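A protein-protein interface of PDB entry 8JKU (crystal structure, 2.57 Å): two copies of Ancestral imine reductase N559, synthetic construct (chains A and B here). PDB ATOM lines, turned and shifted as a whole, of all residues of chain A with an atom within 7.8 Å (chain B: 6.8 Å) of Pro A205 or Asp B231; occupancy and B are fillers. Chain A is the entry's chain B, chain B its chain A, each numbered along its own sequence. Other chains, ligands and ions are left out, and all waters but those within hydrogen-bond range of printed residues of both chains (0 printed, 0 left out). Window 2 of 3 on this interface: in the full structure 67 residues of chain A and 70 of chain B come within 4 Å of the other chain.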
ATOM      1  N   TYR A 192      -3.016  -6.281 -34.066  1.00  0.00           N
ATOM      2  CA  TYR A 192      -2.644  -4.990 -33.500  1.00  0.00           C
ATOM      3  C   TYR A 192      -3.870  -4.239 -33.000  1.00  0.00           C
ATOM      4  O   TYR A 192      -3.854  -3.671 -31.901  1.00  0.00           O
ATOM      5  CB  TYR A 192      -1.896  -4.159 -34.539  1.00  0.00           C
ATOM      6  CG  TYR A 192      -1.491  -2.788 -34.055  1.00  0.00           C
ATOM      7  CD1 TYR A 192      -0.569  -2.638 -33.031  1.00  0.00           C
ATOM      8  CD2 TYR A 192      -2.030  -1.641 -34.623  1.00  0.00           C
ATOM      9  CE1 TYR A 192      -0.195  -1.387 -32.583  1.00  0.00           C
ATOM     10  CE2 TYR A 192      -1.661  -0.384 -34.183  1.00  0.00           C
ATOM     11  CZ  TYR A 192      -0.740  -0.264 -33.163  1.00  0.00           C
ATOM     12  OH  TYR A 192      -0.364   0.980 -32.716  1.00  0.00           O
ATOM     13  N   ALA A 196      -4.635  -3.058 -29.313  1.00  0.00           N
ATOM     14  CA  ALA A 196      -4.944  -1.664 -29.015  1.00  0.00           C
ATOM     15  C   ALA A 196      -6.258  -1.550 -28.255  1.00  0.00           C
ATOM     16  O   ALA A 196      -6.373  -0.760 -27.310  1.00  0.00           O
ATOM     17  CB  ALA A 196      -4.993  -0.847 -30.305  1.00  0.00           C
ATOM     18  N   VAL A 199      -5.568  -2.613 -24.478  1.00  0.00           N
ATOM     19  CA  VAL A 199      -4.970  -1.581 -23.638  1.00  0.00           C
ATOM     20  C   VAL A 199      -5.901  -0.381 -23.525  1.00  0.00           C
ATOM     21  O   VAL A 199      -5.878   0.342 -22.520  1.00  0.00           O
ATOM     22  CB  VAL A 199      -3.588  -1.163 -24.178  1.00  0.00           C
ATOM     23  CG1 VAL A 199      -2.632  -2.349 -24.188  1.00  0.00           C
ATOM     24  CG2 VAL A 199      -3.715  -0.560 -25.568  1.00  0.00           C
ATOM     25  N   GLY A 200      -6.729  -0.141 -24.542  1.00  0.00           N
ATOM     26  CA  GLY A 200      -7.660   0.972 -24.496  1.00  0.00           C
ATOM     27  C   GLY A 200      -8.764   0.812 -23.473  1.00  0.00           C
ATOM     28  O   GLY A 200      -9.313   1.817 -23.008  1.00  0.00           O
ATOM     29  N   GLU A 202      -8.481   0.337 -20.566  1.00  0.00           N
ATOM     30  CA  GLU A 202      -8.025   1.056 -19.384  1.00  0.00           C
ATOM     31  C   GLU A 202      -7.566   2.470 -19.723  1.00  0.00           C
ATOM     32  O   GLU A 202      -6.788   3.066 -18.970  1.00  0.00           O
ATOM     33  CB  GLU A 202      -6.901   0.281 -18.695  1.00  0.00           C
ATOM     34  CG  GLU A 202      -7.338  -1.047 -18.096  1.00  0.00           C
ATOM     35  CD  GLU A 202      -8.350  -0.881 -16.977  1.00  0.00           C
ATOM     36  OE1 GLU A 202      -8.369   0.196 -16.346  1.00  0.00           O
ATOM     37  OE2 GLU A 202      -9.127  -1.828 -16.730  1.00  0.00           O
ATOM     38  N   GLY A 203      -8.024   3.013 -20.849  1.00  0.00           N
ATOM     39  CA  GLY A 203      -7.720   4.376 -21.220  1.00  0.00           C
ATOM     40  C   GLY A 203      -6.393   4.585 -21.914  1.00  0.00           C
ATOM     41  O   GLY A 203      -6.093   5.723 -22.303  1.00  0.00           O
ATOM     42  N   VAL A 204      -5.590   3.543 -22.084  1.00  0.00           N
ATOM     43  CA  VAL A 204      -4.282   3.684 -22.718  1.00  0.00           C
ATOM     44  C   VAL A 204      -4.486   4.187 -24.142  1.00  0.00           C
ATOM     45  O   VAL A 204      -5.169   3.523 -24.937  1.00  0.00           O
ATOM     46  CB  VAL A 204      -3.505   2.359 -22.708  1.00  0.00           C
ATOM     47  CG1 VAL A 204      -2.173   2.529 -23.428  1.00  0.00           C
ATOM     48  CG2 VAL A 204      -3.294   1.873 -21.283  1.00  0.00           C
ATOM     49  N   PRO A 205      -3.932   5.342 -24.511  1.00  0.00           N
ATOM     50  CA  PRO A 205      -4.050   5.792 -25.904  1.00  0.00           C
ATOM     51  C   PRO A 205      -3.261   4.887 -26.837  1.00  0.00           C
ATOM     52  O   PRO A 205      -2.161   4.435 -26.511  1.00  0.00           O
ATOM     53  CB  PRO A 205      -3.474   7.215 -25.883  1.00  0.00           C
ATOM     54  CG  PRO A 205      -3.392   7.602 -24.430  1.00  0.00           C
ATOM     55  CD  PRO A 205      -3.219   6.322 -23.670  1.00  0.00           C
ATOM     56  N   ALA A 206      -3.839   4.622 -28.011  1.00  0.00           N
ATOM     57  CA  ALA A 206      -3.150   3.795 -28.995  1.00  0.00           C
ATOM     58  C   ALA A 206      -1.779   4.361 -29.339  1.00  0.00           C
ATOM     59  O   ALA A 206      -0.863   3.605 -29.682  1.00  0.00           O
ATOM     60  CB  ALA A 206      -4.004   3.664 -30.256  1.00  0.00           C
ATOM     61  N   ALA A 207      -1.616   5.684 -29.250  1.00  0.00           N
ATOM     62  CA  ALA A 207      -0.324   6.290 -29.553  1.00  0.00           C
ATOM     63  C   ALA A 207       0.715   5.964 -28.489  1.00  0.00           C
ATOM     64  O   ALA A 207       1.916   5.951 -28.782  1.00  0.00           O
ATOM     65  CB  ALA A 207      -0.478   7.804 -29.698  1.00  0.00           C
ATOM     66  N   GLU A 208       0.281   5.709 -27.252  1.00  0.00           N
ATOM     67  CA  GLU A 208       1.211   5.282 -26.213  1.00  0.00           C
ATOM     68  C   GLU A 208       1.597   3.818 -26.368  1.00  0.00           C
ATOM     69  O   GLU A 208       2.683   3.415 -25.935  1.00  0.00           O
ATOM     70  CB  GLU A 208       0.599   5.506 -24.830  1.00  0.00           C
ATOM     71  CG  GLU A 208       0.223   6.946 -24.541  1.00  0.00           C
ATOM     72  CD  GLU A 208       0.409   7.311 -23.081  1.00  0.00           C
ATOM     73  OE1 GLU A 208       0.597   8.510 -22.788  1.00  0.00           O
ATOM     74  OE2 GLU A 208       0.366   6.401 -22.227  1.00  0.00           O
ATOM     75  N   PHE A 209       0.726   3.012 -26.979  1.00  0.00           N
ATOM     76  CA  PHE A 209       1.004   1.590 -27.139  1.00  0.00           C
ATOM     77  C   PHE A 209       1.856   1.323 -28.373  1.00  0.00           C
ATOM     78  O   PHE A 209       2.712   0.432 -28.357  1.00  0.00           O
ATOM     79  CB  PHE A 209      -0.312   0.815 -27.218  1.00  0.00           C
ATOM     80  CG  PHE A 209      -0.140  -0.674 -27.281  1.00  0.00           C
ATOM     81  CD1 PHE A 209       0.345  -1.375 -26.192  1.00  0.00           C
ATOM     82  CD2 PHE A 209      -0.467  -1.374 -28.429  1.00  0.00           C
ATOM     83  CE1 PHE A 209       0.503  -2.744 -26.249  1.00  0.00           C
ATOM     84  CE2 PHE A 209      -0.311  -2.742 -28.490  1.00  0.00           C
ATOM     85  CZ  PHE A 209       0.173  -3.429 -27.398  1.00  0.00           C
ATOM     86  N   ALA A 210       1.643   2.092 -29.440  1.00  0.00           N
ATOM     87  CA  ALA A 210       2.362   1.867 -30.693  1.00  0.00           C
ATOM     88  C   ALA A 210       3.865   1.719 -30.507  1.00  0.00           C
ATOM     89  O   ALA A 210       4.447   0.792 -31.092  1.00  0.00           O
ATOM     90  CB  ALA A 210       2.044   3.010 -31.665  1.00  0.00           C
ATOM     91  N   PRO A 211       4.545   2.563 -29.725  1.00  0.00           N
ATOM     92  CA  PRO A 211       6.001   2.386 -29.575  1.00  0.00           C
ATOM     93  C   PRO A 211       6.385   1.020 -29.034  1.00  0.00           C
ATOM     94  O   PRO A 211       7.399   0.450 -29.459  1.00  0.00           O
ATOM     95  CB  PRO A 211       6.397   3.513 -28.608  1.00  0.00           C
ATOM     96  CG  PRO A 211       5.288   4.523 -28.710  1.00  0.00           C
ATOM     97  CD  PRO A 211       4.040   3.731 -28.980  1.00  0.00           C
ATOM     98  N   PHE A 212       5.601   0.476 -28.100  1.00  0.00           N
ATOM     99  CA  PHE A 212       5.931  -0.830 -27.537  1.00  0.00           C
ATOM    100  C   PHE A 212       5.610  -1.947 -28.519  1.00  0.00           C
ATOM    101  O   PHE A 212       6.387  -2.899 -28.660  1.00  0.00           O
ATOM    102  CB  PHE A 212       5.178  -1.039 -26.225  1.00  0.00           C
ATOM    103  CG  PHE A 212       5.474   0.003 -25.189  1.00  0.00           C
ATOM    104  CD1 PHE A 212       6.624  -0.072 -24.422  1.00  0.00           C
ATOM    105  CD2 PHE A 212       4.604   1.060 -24.986  1.00  0.00           C
ATOM    106  CE1 PHE A 212       6.899   0.887 -23.467  1.00  0.00           C
ATOM    107  CE2 PHE A 212       4.873   2.021 -24.033  1.00  0.00           C
ATOM    108  CZ  PHE A 212       6.022   1.935 -23.273  1.00  0.00           C
ATOM    109  N   TYR B 177      -0.521  -4.499 -20.551  1.00  0.00           N
ATOM    110  CA  TYR B 177       0.459  -4.345 -21.621  1.00  0.00           C
ATOM    111  C   TYR B 177       1.036  -5.696 -22.023  1.00  0.00           C
ATOM    112  O   TYR B 177       1.308  -5.940 -23.204  1.00  0.00           O
ATOM    113  CB  TYR B 177       1.583  -3.408 -21.177  1.00  0.00           C
ATOM    114  CG  TYR B 177       1.276  -1.935 -21.318  1.00  0.00           C
ATOM    115  CD1 TYR B 177       0.233  -1.351 -20.613  1.00  0.00           C
ATOM    116  CD2 TYR B 177       2.042  -1.124 -22.146  1.00  0.00           C
ATOM    117  CE1 TYR B 177      -0.043  -0.003 -20.732  1.00  0.00           C
ATOM    118  CE2 TYR B 177       1.771   0.225 -22.274  1.00  0.00           C
ATOM    119  CZ  TYR B 177       0.728   0.780 -21.565  1.00  0.00           C
ATOM    120  OH  TYR B 177       0.455   2.122 -21.687  1.00  0.00           O
ATOM    121  N   MET B 226      -2.103   4.066 -37.769  1.00  0.00           N
ATOM    122  CA  MET B 226      -3.426   3.621 -37.341  1.00  0.00           C
ATOM    123  C   MET B 226      -3.750   4.100 -35.933  1.00  0.00           C
ATOM    124  O   MET B 226      -4.919   4.349 -35.620  1.00  0.00           O
ATOM    125  CB  MET B 226      -3.515   2.096 -37.405  1.00  0.00           C
ATOM    126  CG  MET B 226      -3.167   1.506 -38.759  1.00  0.00           C
ATOM    127  SD  MET B 226      -2.708  -0.234 -38.644  1.00  0.00           S
ATOM    128  CE  MET B 226      -4.295  -0.990 -38.296  1.00  0.00           C
ATOM    129  N   ALA B 227      -2.738   4.225 -35.071  1.00  0.00           N
ATOM    130  CA  ALA B 227      -2.980   4.736 -33.726  1.00  0.00           C
ATOM    131  C   ALA B 227      -3.566   6.140 -33.767  1.00  0.00           C
ATOM    132  O   ALA B 227      -4.378   6.500 -32.907  1.00  0.00           O
ATOM    133  CB  ALA B 227      -1.684   4.725 -32.915  1.00  0.00           C
ATOM    134  N   GLU B 228      -3.167   6.946 -34.755  1.00  0.00           N
ATOM    135  CA  GLU B 228      -3.749   8.275 -34.905  1.00  0.00           C
ATOM    136  C   GLU B 228      -5.231   8.186 -35.246  1.00  0.00           C
ATOM    137  O   GLU B 228      -6.042   8.966 -34.734  1.00  0.00           O
ATOM    138  CB  GLU B 228      -2.996   9.054 -35.981  1.00  0.00           C
ATOM    139  CG  GLU B 228      -1.589   9.463 -35.580  1.00  0.00           C
ATOM    140  CD  GLU B 228      -1.441  10.965 -35.424  1.00  0.00           C
ATOM    141  OE1 GLU B 228      -0.810  11.402 -34.437  1.00  0.00           O
ATOM    142  OE2 GLU B 228      -1.951  11.709 -36.287  1.00  0.00           O
ATOM    143  N   GLN B 229      -5.603   7.239 -36.109  1.00  0.00           N
ATOM    144  CA  GLN B 229      -7.013   7.041 -36.427  1.00  0.00           C
ATOM    145  C   GLN B 229      -7.786   6.564 -35.206  1.00  0.00           C
ATOM    146  O   GLN B 229      -8.870   7.076 -34.903  1.00  0.00           O
ATOM    147  CB  GLN B 229      -7.156   6.036 -37.568  1.00  0.00           C
ATOM    148  CG  GLN B 229      -6.891   6.601 -38.946  1.00  0.00           C
ATOM    149  CD  GLN B 229      -6.907   5.531 -40.016  1.00  0.00           C
ATOM    150  OE1 GLN B 229      -7.873   5.405 -40.769  1.00  0.00           O
ATOM    151  NE2 GLN B 229      -5.836   4.747 -40.086  1.00  0.00           N
ATOM    152  N   ILE B 230      -7.242   5.575 -34.493  1.00  0.00           N
ATOM    153  CA  ILE B 230      -7.930   5.023 -33.330  1.00  0.00           C
ATOM    154  C   ILE B 230      -8.157   6.109 -32.287  1.00  0.00           C
ATOM    155  O   ILE B 230      -9.257   6.253 -31.741  1.00  0.00           O
ATOM    156  CB  ILE B 230      -7.130   3.846 -32.744  1.00  0.00           C
ATOM    157  CG1 ILE B 230      -7.020   2.712 -33.762  1.00  0.00           C
ATOM    158  CG2 ILE B 230      -7.782   3.352 -31.464  1.00  0.00           C
ATOM    159  CD1 ILE B 230      -5.808   1.825 -33.560  1.00  0.00           C
ATOM    160  N   ASP B 231      -7.112   6.883 -31.988  1.00  0.00           N
ATOM    161  CA  ASP B 231      -7.236   7.929 -30.981  1.00  0.00           C
ATOM    162  C   ASP B 231      -8.175   9.037 -31.440  1.00  0.00           C
ATOM    163  O   ASP B 231      -8.888   9.625 -30.618  1.00  0.00           O
ATOM    164  CB  ASP B 231      -5.857   8.499 -30.647  1.00  0.00           C
ATOM    165  CG  ASP B 231      -4.968   7.497 -29.921  1.00  0.00           C
ATOM    166  OD1 ASP B 231      -5.502   6.639 -29.185  1.00  0.00           O
ATOM    167  OD2 ASP B 231      -3.731   7.570 -30.086  1.00  0.00           O
ATOM    168  N   ALA B 232      -8.198   9.331 -32.740  1.00  0.00           N
ATOM    169  CA  ALA B 232      -9.095  10.346 -33.274  1.00  0.00           C
ATOM    170  C   ALA B 232     -10.508   9.828 -33.503  1.00  0.00           C
ATOM    171  O   ALA B 232     -11.405  10.630 -33.783  1.00  0.00           O
ATOM    172  CB  ALA B 232      -8.540  10.895 -34.591  1.00  0.00           C
ATOM    173  N   GLY B 233     -10.729   8.521 -33.389  1.00  0.00           N
ATOM    174  CA  GLY B 233     -12.035   7.967 -33.688  1.00  0.00           C
ATOM    175  C   GLY B 233     -12.514   8.240 -35.092  1.00  0.00           C
ATOM    176  O   GLY B 233     -13.719   8.180 -35.351  1.00  0.00           O
ATOM    177  N   GLU B 234     -11.600   8.546 -36.011  1.00  0.00           N
ATOM    178  CA  GLU B 234     -11.929   8.840 -37.400  1.00  0.00           C
ATOM    179  C   GLU B 234     -11.112   7.914 -38.286  1.00  0.00           C
ATOM    180  O   GLU B 234      -9.880   7.899 -38.203  1.00  0.00           O
ATOM    181  CB  GLU B 234     -11.644  10.304 -37.738  1.00  0.00           C
ATOM    182  CG  GLU B 234     -12.442  11.297 -36.906  1.00  0.00           C
ATOM    183  CD  GLU B 234     -13.493  12.027 -37.720  1.00  0.00           C
ATOM    184  OE1 GLU B 234     -14.308  11.352 -38.384  1.00  0.00           O
ATOM    185  OE2 GLU B 234     -13.505  13.276 -37.691  1.00  0.00           O
ATOM    186  N   TYR B 235     -11.784   7.071 -39.073  1.00  0.00           N
ATOM    187  CA  TYR B 235     -11.128   6.055 -39.932  1.00  0.00           C
ATOM    188  C   TYR B 235     -11.331   6.424 -41.404  1.00  0.00           C
ATOM    189  O   TYR B 235     -12.174   5.824 -42.078  1.00  0.00           O
ATOM    190  CB  TYR B 235     -11.690   4.679 -39.581  1.00  0.00           C
ATOM    191  CG  TYR B 235     -11.785   4.423 -38.102  1.00  0.00           C
ATOM    192  CD1 TYR B 235     -10.648   4.314 -37.320  1.00  0.00           C
ATOM    193  CD2 TYR B 235     -13.014   4.313 -37.479  1.00  0.00           C
ATOM    194  CE1 TYR B 235     -10.730   4.090 -35.957  1.00  0.00           C
ATOM    195  CE2 TYR B 235     -13.115   4.089 -36.118  1.00  0.00           C
ATOM    196  CZ  TYR B 235     -11.970   3.976 -35.355  1.00  0.00           C
ATOM    197  OH  TYR B 235     -12.088   3.754 -34.007  1.00  0.00           O
ATOM    198  N   ARG B 294     -14.170  -3.731 -29.700  1.00  0.00           N
ATOM    199  CA  ARG B 294     -14.520  -3.265 -28.366  1.00  0.00           C
ATOM    200  C   ARG B 294     -15.881  -3.769 -27.895  1.00  0.00           C
ATOM    201  O   ARG B 294     -16.331  -3.367 -26.816  1.00  0.00           O
ATOM    202  CB  ARG B 294     -14.503  -1.734 -28.328  1.00  0.00           C
ATOM    203  CG  ARG B 294     -13.131  -1.117 -28.556  1.00  0.00           C
ATOM    204  CD  ARG B 294     -13.081   0.325 -28.068  1.00  0.00           C
ATOM    205  NE  ARG B 294     -12.615   1.245 -29.100  1.00  0.00           N
ATOM    206  CZ  ARG B 294     -11.365   1.673 -29.216  1.00  0.00           C
ATOM    207  NH1 ARG B 294     -10.416   1.274 -28.385  1.00  0.00           N
ATOM    208  NH2 ARG B 294     -11.059   2.524 -30.192  1.00  0.00           N
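OD2 of Asp B231 lies within hydrogen-bond range of N of Ala A207. The backbone NH (N) of Ala A206 lies within hydrogen-bond range of the side-chain carboxylate (OD1) of Asp B231 (2.9 Å).
The backbone NH (N) of Val A204 lies close to the backbone carbonyl oxygen (O) of Val A199 (3.2 Å).
Among the printed residues, merely in contact across the chains: Tyr A192 with Ala B227 (3.98 Å), Val A204 with Tyr B177 (3.2 Å), Pro A205 with Asp B231 (3.7 Å), Ala A206 with Ala B227 (3.5 Å), Ala A206 with Ile B230 (3.98 Å), Ala A207 with Ala B227 (3.8 Å) and Phe A212 with Tyr B177 (3.99 Å).
Of chain B, only Asp B231 comes within 4 Å of Pro A205. Asp B231 touches three residues of chain A. Printed residues of chain A within 4 Å of Ile B230: Ala A206 (3.98 Å). Of the printed residues of chain B, Val A204 touches Tyr B177 (3.2 Å). Printed residues of chain B within 4 Å of Phe A212: Tyr B177 (3.99 Å). Of the printed residues of chain B, Tyr A192 touches Ala B227 (3.98 Å). Printed residues of chain A within 4 Å of Tyr B177: Val A204 and Phe A212. Arg B294 touches none of the printed residues of chain A. The nearest residue of chain B that does not touch Pro A205 is Tyr B177 (5.9 Å).
Hydrophobic or aromatic side chains of chain B that line the printed part of chain A: Tyr B177, Ala B227 and Ile B230. Printed residues of chain A that touch a printed residue of chain B: Tyr A192, Val A204, Pro A205, Ala A206, Ala A207 and Phe A212. Hydrophobic or aromatic side chains of chain A that line the printed part of chain B: Tyr A192, Val A204, Pro A205, Ala A206, Ala A207 and Phe A212. Among the printed residues, no Asp or Glu carboxylate lies within 4 Å of a Lys or Arg side-chain nitrogen of the other chain.
No position is printed for both chains.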
